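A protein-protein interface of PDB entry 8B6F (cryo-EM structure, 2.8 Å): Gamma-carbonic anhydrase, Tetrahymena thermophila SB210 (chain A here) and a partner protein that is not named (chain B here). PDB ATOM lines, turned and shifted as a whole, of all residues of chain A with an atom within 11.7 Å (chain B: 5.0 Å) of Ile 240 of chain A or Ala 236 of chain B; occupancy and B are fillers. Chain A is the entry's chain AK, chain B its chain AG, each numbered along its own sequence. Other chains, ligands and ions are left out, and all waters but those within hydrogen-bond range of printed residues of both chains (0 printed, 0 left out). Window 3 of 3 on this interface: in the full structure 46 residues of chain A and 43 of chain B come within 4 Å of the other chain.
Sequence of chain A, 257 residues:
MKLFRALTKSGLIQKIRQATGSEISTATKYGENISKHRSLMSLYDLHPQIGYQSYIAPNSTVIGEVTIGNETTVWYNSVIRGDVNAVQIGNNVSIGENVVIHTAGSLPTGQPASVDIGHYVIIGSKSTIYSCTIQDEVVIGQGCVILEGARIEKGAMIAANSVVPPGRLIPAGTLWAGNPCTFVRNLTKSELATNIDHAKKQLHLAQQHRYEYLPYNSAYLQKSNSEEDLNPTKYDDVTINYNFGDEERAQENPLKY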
ATOM      1  N   TYR A  44      11.946   2.524  11.309  1.00  0.00           N
ATOM      2  CA  TYR A  44      10.792   1.634  11.241  1.00  0.00           C
ATOM      3  C   TYR A  44      10.821   0.501  12.259  1.00  0.00           C
ATOM      4  O   TYR A  44       9.775  -0.086  12.556  1.00  0.00           O
ATOM      5  CB  TYR A  44      10.681   0.997   9.849  1.00  0.00           C
ATOM      6  CG  TYR A  44      10.963   1.916   8.682  1.00  0.00           C
ATOM      7  CD1 TYR A  44      10.633   3.265   8.730  1.00  0.00           C
ATOM      8  CD2 TYR A  44      11.552   1.425   7.524  1.00  0.00           C
ATOM      9  CE1 TYR A  44      10.891   4.100   7.661  1.00  0.00           C
ATOM     10  CE2 TYR A  44      11.813   2.248   6.451  1.00  0.00           C
ATOM     11  CZ  TYR A  44      11.481   3.587   6.525  1.00  0.00           C
ATOM     12  OH  TYR A  44      11.737   4.417   5.458  1.00  0.00           O
ATOM     13  N   ASP A  45      11.986   0.191  12.815  1.00  0.00           N
ATOM     14  CA  ASP A  45      12.055  -0.717  13.952  1.00  0.00           C
ATOM     15  C   ASP A  45      13.215  -0.428  14.888  1.00  0.00           C
ATOM     16  O   ASP A  45      13.375  -1.158  15.870  1.00  0.00           O
ATOM     17  CB  ASP A  45      12.142  -2.166  13.455  1.00  0.00           C
ATOM     18  CG  ASP A  45      10.836  -2.661  12.874  1.00  0.00           C
ATOM     19  OD1 ASP A  45       9.784  -2.453  13.514  1.00  0.00           O
ATOM     20  OD2 ASP A  45      10.860  -3.247  11.772  1.00  0.00           O
ATOM     21  N   HIS A  47      15.003   1.808  17.362  1.00  0.00           N
ATOM     22  CA  HIS A  47      14.851   2.927  18.272  1.00  0.00           C
ATOM     23  C   HIS A  47      16.108   3.075  19.110  1.00  0.00           C
ATOM     24  O   HIS A  47      16.462   2.134  19.837  1.00  0.00           O
ATOM     25  CB  HIS A  47      13.641   2.708  19.167  1.00  0.00           C
ATOM     26  CG  HIS A  47      12.460   2.149  18.440  1.00  0.00           C
ATOM     27  ND1 HIS A  47      11.810   2.835  17.437  1.00  0.00           N
ATOM     28  CD2 HIS A  47      11.818   0.965  18.562  1.00  0.00           C
ATOM     29  CE1 HIS A  47      10.817   2.099  16.976  1.00  0.00           C
ATOM     30  NE2 HIS A  47      10.799   0.959  17.641  1.00  0.00           N
ATOM     31  N   ASP A 236      -6.516  11.687  12.591  1.00  0.00           N
ATOM     32  CA  ASP A 236      -6.208  10.349  13.068  1.00  0.00           C
ATOM     33  C   ASP A 236      -7.043  10.031  14.300  1.00  0.00           C
ATOM     34  O   ASP A 236      -7.607  10.919  14.945  1.00  0.00           O
ATOM     35  CB  ASP A 236      -4.720  10.211  13.404  1.00  0.00           C
ATOM     36  CG  ASP A 236      -3.827  10.421  12.198  1.00  0.00           C
ATOM     37  OD1 ASP A 236      -4.227  10.026  11.083  1.00  0.00           O
ATOM     38  OD2 ASP A 236      -2.723  10.976  12.364  1.00  0.00           O
ATOM     39  N   ASP A 237      -7.120   8.742  14.620  1.00  0.00           N
ATOM     40  CA  ASP A 237      -7.839   8.282  15.798  1.00  0.00           C
ATOM     41  C   ASP A 237      -6.924   8.330  17.014  1.00  0.00           C
ATOM     42  O   ASP A 237      -5.758   7.931  16.946  1.00  0.00           O
ATOM     43  CB  ASP A 237      -8.365   6.861  15.589  1.00  0.00           C
ATOM     44  CG  ASP A 237      -9.300   6.419  16.697  1.00  0.00           C
ATOM     45  OD1 ASP A 237     -10.374   7.035  16.849  1.00  0.00           O
ATOM     46  OD2 ASP A 237      -8.964   5.455  17.414  1.00  0.00           O
ATOM     47  N   VAL A 238      -7.456   8.829  18.126  1.00  0.00           N
ATOM     48  CA  VAL A 238      -6.670   8.970  19.349  1.00  0.00           C
ATOM     49  C   VAL A 238      -6.375   7.576  19.896  1.00  0.00           C
ATOM     50  O   VAL A 238      -7.277   6.868  20.353  1.00  0.00           O
ATOM     51  CB  VAL A 238      -7.385   9.849  20.384  1.00  0.00           C
ATOM     52  CG1 VAL A 238      -7.580  11.252  19.839  1.00  0.00           C
ATOM     53  CG2 VAL A 238      -8.733   9.264  20.797  1.00  0.00           C
ATOM     54  N   THR A 239      -5.111   7.162  19.816  1.00  0.00           N
ATOM     55  CA  THR A 239      -4.670   5.880  20.354  1.00  0.00           C
ATOM     56  C   THR A 239      -3.963   6.044  21.695  1.00  0.00           C
ATOM     57  O   THR A 239      -4.429   5.529  22.714  1.00  0.00           O
ATOM     58  CB  THR A 239      -3.744   5.178  19.351  1.00  0.00           C
ATOM     59  OG1 THR A 239      -2.582   5.984  19.117  1.00  0.00           O
ATOM     60  CG2 THR A 239      -4.466   4.935  18.036  1.00  0.00           C
ATOM     61  N   ILE A 240      -2.847   6.763  21.712  1.00  0.00           N
ATOM     62  CA  ILE A 240      -2.093   6.990  22.938  1.00  0.00           C
ATOM     63  C   ILE A 240      -1.148   8.157  22.696  1.00  0.00           C
ATOM     64  O   ILE A 240      -0.599   8.311  21.603  1.00  0.00           O
ATOM     65  CB  ILE A 240      -1.332   5.713  23.373  1.00  0.00           C
ATOM     66  CG1 ILE A 240      -0.613   5.926  24.708  1.00  0.00           C
ATOM     67  CG2 ILE A 240      -0.324   5.300  22.311  1.00  0.00           C
ATOM     68  CD1 ILE A 240      -1.541   6.117  25.880  1.00  0.00           C
ATOM     69  N   ASN A 241      -0.960   8.974  23.726  1.00  0.00           N
ATOM     70  CA  ASN A 241      -0.016  10.079  23.670  1.00  0.00           C
ATOM     71  C   ASN A 241       1.352   9.577  24.101  1.00  0.00           C
ATOM     72  O   ASN A 241       1.484   8.940  25.150  1.00  0.00           O
ATOM     73  CB  ASN A 241      -0.466  11.228  24.570  1.00  0.00           C
ATOM     74  CG  ASN A 241      -1.691  11.938  24.041  1.00  0.00           C
ATOM     75  OD1 ASN A 241      -2.373  11.442  23.147  1.00  0.00           O
ATOM     76  ND2 ASN A 241      -1.981  13.107  24.597  1.00  0.00           N
ATOM     77  N   TYR A 242       2.369   9.862  23.287  1.00  0.00           N
ATOM     78  CA  TYR A 242       3.706   9.378  23.605  1.00  0.00           C
ATOM     79  C   TYR A 242       4.158   9.850  24.978  1.00  0.00           C
ATOM     80  O   TYR A 242       4.933   9.159  25.647  1.00  0.00           O
ATOM     81  CB  TYR A 242       4.701   9.824  22.534  1.00  0.00           C
ATOM     82  CG  TYR A 242       5.068  11.285  22.611  1.00  0.00           C
ATOM     83  CD1 TYR A 242       4.226  12.263  22.103  1.00  0.00           C
ATOM     84  CD2 TYR A 242       6.265  11.686  23.188  1.00  0.00           C
ATOM     85  CE1 TYR A 242       4.562  13.599  22.175  1.00  0.00           C
ATOM     86  CE2 TYR A 242       6.610  13.017  23.264  1.00  0.00           C
ATOM     87  CZ  TYR A 242       5.756  13.969  22.755  1.00  0.00           C
ATOM     88  OH  TYR A 242       6.100  15.297  22.830  1.00  0.00           O
ATOM     89  N   ASN A 243       3.691  11.015  25.411  1.00  0.00           N
ATOM     90  CA  ASN A 243       4.020  11.552  26.730  1.00  0.00           C
ATOM     91  C   ASN A 243       2.913  11.221  27.729  1.00  0.00           C
ATOM     92  O   ASN A 243       2.335  12.093  28.376  1.00  0.00           O
ATOM     93  CB  ASN A 243       4.254  13.055  26.641  1.00  0.00           C
ATOM     94  CG  ASN A 243       3.022  13.807  26.190  1.00  0.00           C
ATOM     95  OD1 ASN A 243       2.179  13.268  25.475  1.00  0.00           O
ATOM     96  ND2 ASN A 243       2.908  15.060  26.610  1.00  0.00           N
ATOM     97  N   PHE A 244       2.619   9.930  27.849  1.00  0.00           N
ATOM     98  CA  PHE A 244       1.626   9.448  28.798  1.00  0.00           C
ATOM     99  C   PHE A 244       2.320   9.146  30.118  1.00  0.00           C
ATOM    100  O   PHE A 244       3.282   8.372  30.156  1.00  0.00           O
ATOM    101  CB  PHE A 244       0.915   8.204  28.265  1.00  0.00           C
ATOM    102  CG  PHE A 244      -0.219   7.736  29.132  1.00  0.00           C
ATOM    103  CD1 PHE A 244      -1.414   8.434  29.171  1.00  0.00           C
ATOM    104  CD2 PHE A 244      -0.093   6.590  29.901  1.00  0.00           C
ATOM    105  CE1 PHE A 244      -2.460   8.002  29.967  1.00  0.00           C
ATOM    106  CE2 PHE A 244      -1.135   6.153  30.699  1.00  0.00           C
ATOM    107  CZ  PHE A 244      -2.320   6.860  30.732  1.00  0.00           C
ATOM    108  N   GLY A 245       1.834   9.755  31.194  1.00  0.00           N
ATOM    109  CA  GLY A 245       2.497   9.657  32.474  1.00  0.00           C
ATOM    110  C   GLY A 245       3.698  10.558  32.633  1.00  0.00           C
ATOM    111  O   GLY A 245       4.448  10.396  33.602  1.00  0.00           O
ATOM    112  N   ASP A 246       3.910  11.502  31.713  1.00  0.00           N
ATOM    113  CA  ASP A 246       5.045  12.410  31.826  1.00  0.00           C
ATOM    114  C   ASP A 246       4.854  13.443  32.925  1.00  0.00           C
ATOM    115  O   ASP A 246       5.827  14.091  33.323  1.00  0.00           O
ATOM    116  CB  ASP A 246       5.303  13.110  30.492  1.00  0.00           C
ATOM    117  CG  ASP A 246       6.120  12.258  29.540  1.00  0.00           C
ATOM    118  OD1 ASP A 246       6.307  11.056  29.822  1.00  0.00           O
ATOM    119  OD2 ASP A 246       6.590  12.793  28.515  1.00  0.00           O
ATOM    120  N   GLU A 247       3.629  13.619  33.421  1.00  0.00           N
ATOM    121  CA  GLU A 247       3.438  14.449  34.604  1.00  0.00           C
ATOM    122  C   GLU A 247       4.030  13.794  35.844  1.00  0.00           C
ATOM    123  O   GLU A 247       4.211  14.470  36.861  1.00  0.00           O
ATOM    124  CB  GLU A 247       1.949  14.748  34.817  1.00  0.00           C
ATOM    125  CG  GLU A 247       1.118  13.609  35.401  1.00  0.00           C
ATOM    126  CD  GLU A 247       1.006  12.418  34.474  1.00  0.00           C
ATOM    127  OE1 GLU A 247       1.439  12.529  33.309  1.00  0.00           O
ATOM    128  OE2 GLU A 247       0.484  11.370  34.910  1.00  0.00           O
ATOM    129  N   ASP B 232       3.746   8.293  18.693  1.00  0.00           N
ATOM    130  CA  ASP B 232       2.594   7.617  19.279  1.00  0.00           C
ATOM    131  C   ASP B 232       2.599   6.131  18.946  1.00  0.00           C
ATOM    132  O   ASP B 232       2.288   5.293  19.799  1.00  0.00           O
ATOM    133  CB  ASP B 232       1.300   8.266  18.794  1.00  0.00           C
ATOM    134  CG  ASP B 232       1.146   9.688  19.280  1.00  0.00           C
ATOM    135  OD1 ASP B 232       2.061  10.184  19.968  1.00  0.00           O
ATOM    136  OD2 ASP B 232       0.107  10.311  18.981  1.00  0.00           O
ATOM    137  N   ARG B 233       2.945   5.784  17.704  1.00  0.00           N
ATOM    138  CA  ARG B 233       2.975   4.380  17.308  1.00  0.00           C
ATOM    139  C   ARG B 233       4.040   3.608  18.076  1.00  0.00           C
ATOM    140  O   ARG B 233       3.803   2.473  18.503  1.00  0.00           O
ATOM    141  CB  ARG B 233       3.214   4.263  15.804  1.00  0.00           C
ATOM    142  CG  ARG B 233       2.984   2.861  15.259  1.00  0.00           C
ATOM    143  CD  ARG B 233       3.612   2.668  13.891  1.00  0.00           C
ATOM    144  NE  ARG B 233       5.069   2.749  13.949  1.00  0.00           N
ATOM    145  CZ  ARG B 233       5.790   3.794  13.565  1.00  0.00           C
ATOM    146  NH1 ARG B 233       5.230   4.877  13.053  1.00  0.00           N
ATOM    147  NH2 ARG B 233       7.113   3.748  13.696  1.00  0.00           N
ATOM    148  N   ILE B 234       5.217   4.204  18.268  1.00  0.00           N
ATOM    149  CA  ILE B 234       6.266   3.530  19.027  1.00  0.00           C
ATOM    150  C   ILE B 234       5.823   3.314  20.469  1.00  0.00           C
ATOM    151  O   ILE B 234       6.039   2.243  21.047  1.00  0.00           O
ATOM    152  CB  ILE B 234       7.577   4.333  18.950  1.00  0.00           C
ATOM    153  CG1 ILE B 234       8.080   4.390  17.507  1.00  0.00           C
ATOM    154  CG2 ILE B 234       8.640   3.720  19.856  1.00  0.00           C
ATOM    155  CD1 ILE B 234       9.215   5.368  17.286  1.00  0.00           C
ATOM    156  N   THR B 235       5.215   4.332  21.079  1.00  0.00           N
ATOM    157  CA  THR B 235       4.733   4.187  22.447  1.00  0.00           C
ATOM    158  C   THR B 235       3.679   3.092  22.544  1.00  0.00           C
ATOM    159  O   THR B 235       3.683   2.296  23.489  1.00  0.00           O
ATOM    160  CB  THR B 235       4.195   5.523  22.949  1.00  0.00           C
ATOM    161  OG1 THR B 235       5.260   6.482  22.923  1.00  0.00           O
ATOM    162  CG2 THR B 235       3.647   5.403  24.366  1.00  0.00           C
ATOM    163  N   ALA B 236       2.760   3.040  21.578  1.00  0.00           N
ATOM    164  CA  ALA B 236       1.734   2.004  21.594  1.00  0.00           C
ATOM    165  C   ALA B 236       2.353   0.624  21.424  1.00  0.00           C
ATOM    166  O   ALA B 236       1.984  -0.320  22.130  1.00  0.00           O
ATOM    167  CB  ALA B 236       0.703   2.268  20.497  1.00  0.00           C
ATOM    168  N   GLU B 237       3.305   0.488  20.498  1.00  0.00           N
ATOM    169  CA  GLU B 237       3.962  -0.799  20.299  1.00  0.00           C
ATOM    170  C   GLU B 237       4.722  -1.236  21.541  1.00  0.00           C
ATOM    171  O   GLU B 237       4.887  -2.436  21.778  1.00  0.00           O
ATOM    172  CB  GLU B 237       4.910  -0.728  19.103  1.00  0.00           C
ATOM    173  CG  GLU B 237       4.205  -0.624  17.766  1.00  0.00           C
ATOM    174  CD  GLU B 237       5.176  -0.491  16.613  1.00  0.00           C
ATOM    175  OE1 GLU B 237       6.399  -0.557  16.856  1.00  0.00           O
ATOM    176  OE2 GLU B 237       4.718  -0.320  15.464  1.00  0.00           O
ATOM    177  N   ALA B 238       5.200  -0.283  22.341  1.00  0.00           N
ATOM    178  CA  ALA B 238       5.864  -0.631  23.588  1.00  0.00           C
ATOM    179  C   ALA B 238       4.952  -1.413  24.524  1.00  0.00           C
ATOM    180  O   ALA B 238       5.450  -2.113  25.413  1.00  0.00           O
ATOM    181  CB  ALA B 238       6.366   0.631  24.290  1.00  0.00           C
ATOM    182  N   GLU B 239       3.633  -1.315  24.348  1.00  0.00           N
ATOM    183  CA  GLU B 239       2.682  -1.995  25.215  1.00  0.00           C
ATOM    184  C   GLU B 239       1.759  -2.957  24.479  1.00  0.00           C
ATOM    185  O   GLU B 239       0.967  -3.645  25.133  1.00  0.00           O
ATOM    186  CB  GLU B 239       1.836  -0.967  25.981  1.00  0.00           C
ATOM    187  CG  GLU B 239       1.008  -0.051  25.093  1.00  0.00           C
ATOM    188  CD  GLU B 239       0.216   0.967  25.892  1.00  0.00           C
ATOM    189  OE1 GLU B 239       0.381   1.010  27.129  1.00  0.00           O
ATOM    190  OE2 GLU B 239      -0.570   1.722  25.284  1.00  0.00           O
ATOM    191  N   TYR B 240       1.818  -3.021  23.151  1.00  0.00           N
ATOM    192  CA  TYR B 240       1.011  -3.989  22.424  1.00  0.00           C
ATOM    193  C   TYR B 240       1.454  -5.407  22.768  1.00  0.00           C
ATOM    194  O   TYR B 240       2.631  -5.670  23.023  1.00  0.00           O
ATOM    195  CB  TYR B 240       1.122  -3.764  20.912  1.00  0.00           C
ATOM    196  CG  TYR B 240       0.250  -2.649  20.364  1.00  0.00           C
ATOM    197  CD1 TYR B 240      -1.012  -2.394  20.888  1.00  0.00           C
ATOM    198  CD2 TYR B 240       0.693  -1.859  19.311  1.00  0.00           C
ATOM    199  CE1 TYR B 240      -1.803  -1.380  20.385  1.00  0.00           C
ATOM    200  CE2 TYR B 240      -0.092  -0.843  18.803  1.00  0.00           C
ATOM    201  CZ  TYR B 240      -1.338  -0.610  19.342  1.00  0.00           C
ATOM    202  OH  TYR B 240      -2.120   0.402  18.836  1.00  0.00           O
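Hydrophobic or aromatic side chains of chain A that line the printed part of chain B: His 47, Ile 240 and Tyr 242. Along chain B the printed residues that touch a printed residue of chain A span positions 232 to 236. Among the printed residues, 5 pairs touch across the chains. Among the printed residues, no Asp or Glu carboxylate lies within 4 Å of a Lys or Arg side-chain nitrogen of the other chain.
Of the printed residues of chain A, Ala 236 of chain B touches Ile 240. Printed residues of chain A within 4 Å of Asp 232 of chain B: Ile 240 and Tyr 242. Thr 235 of chain B touches one residue of chain A. No residue of chain A comes within 4 Å of Glu 237 of chain B. No residue of chain A comes within 4 Å of Ala 238 of chain B. No residue of chain A comes within 4 Å of Glu 239 of chain B. No residue of chain A comes within 4 Å of Tyr 240 of chain B. Printed residues of chain B within 4 Å of His 47 of chain A: Ile 234 (3.6 Å). Of the printed residues of chain B, Tyr 242 of chain A touches Asp 232 (3.3 Å) and Thr 235 (3.4 Å). Of the printed residues of chain A, Ile 234 of chain B touches His 47 (3.6 Å). Phe 244 of chain A touches none of the printed residues of chain B.
Among the printed residues, merely in contact across the chains: His 47 of chain A with Ile 234 of chain B, Ile 240 of chain A with Ala 236 of chain B and Tyr 242 of chain A with Thr 235 of chain B.
The side-chain carboxylate (OD2) of Asp 232 of chain B lies close to the backbone carbonyl oxygen (O) of Ile 240 of chain A, 3.4 Å away. OD1 of Asp 232 of chain B is in hydrogen-bond range of N of Tyr 242 of chain A (3.3 Å).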
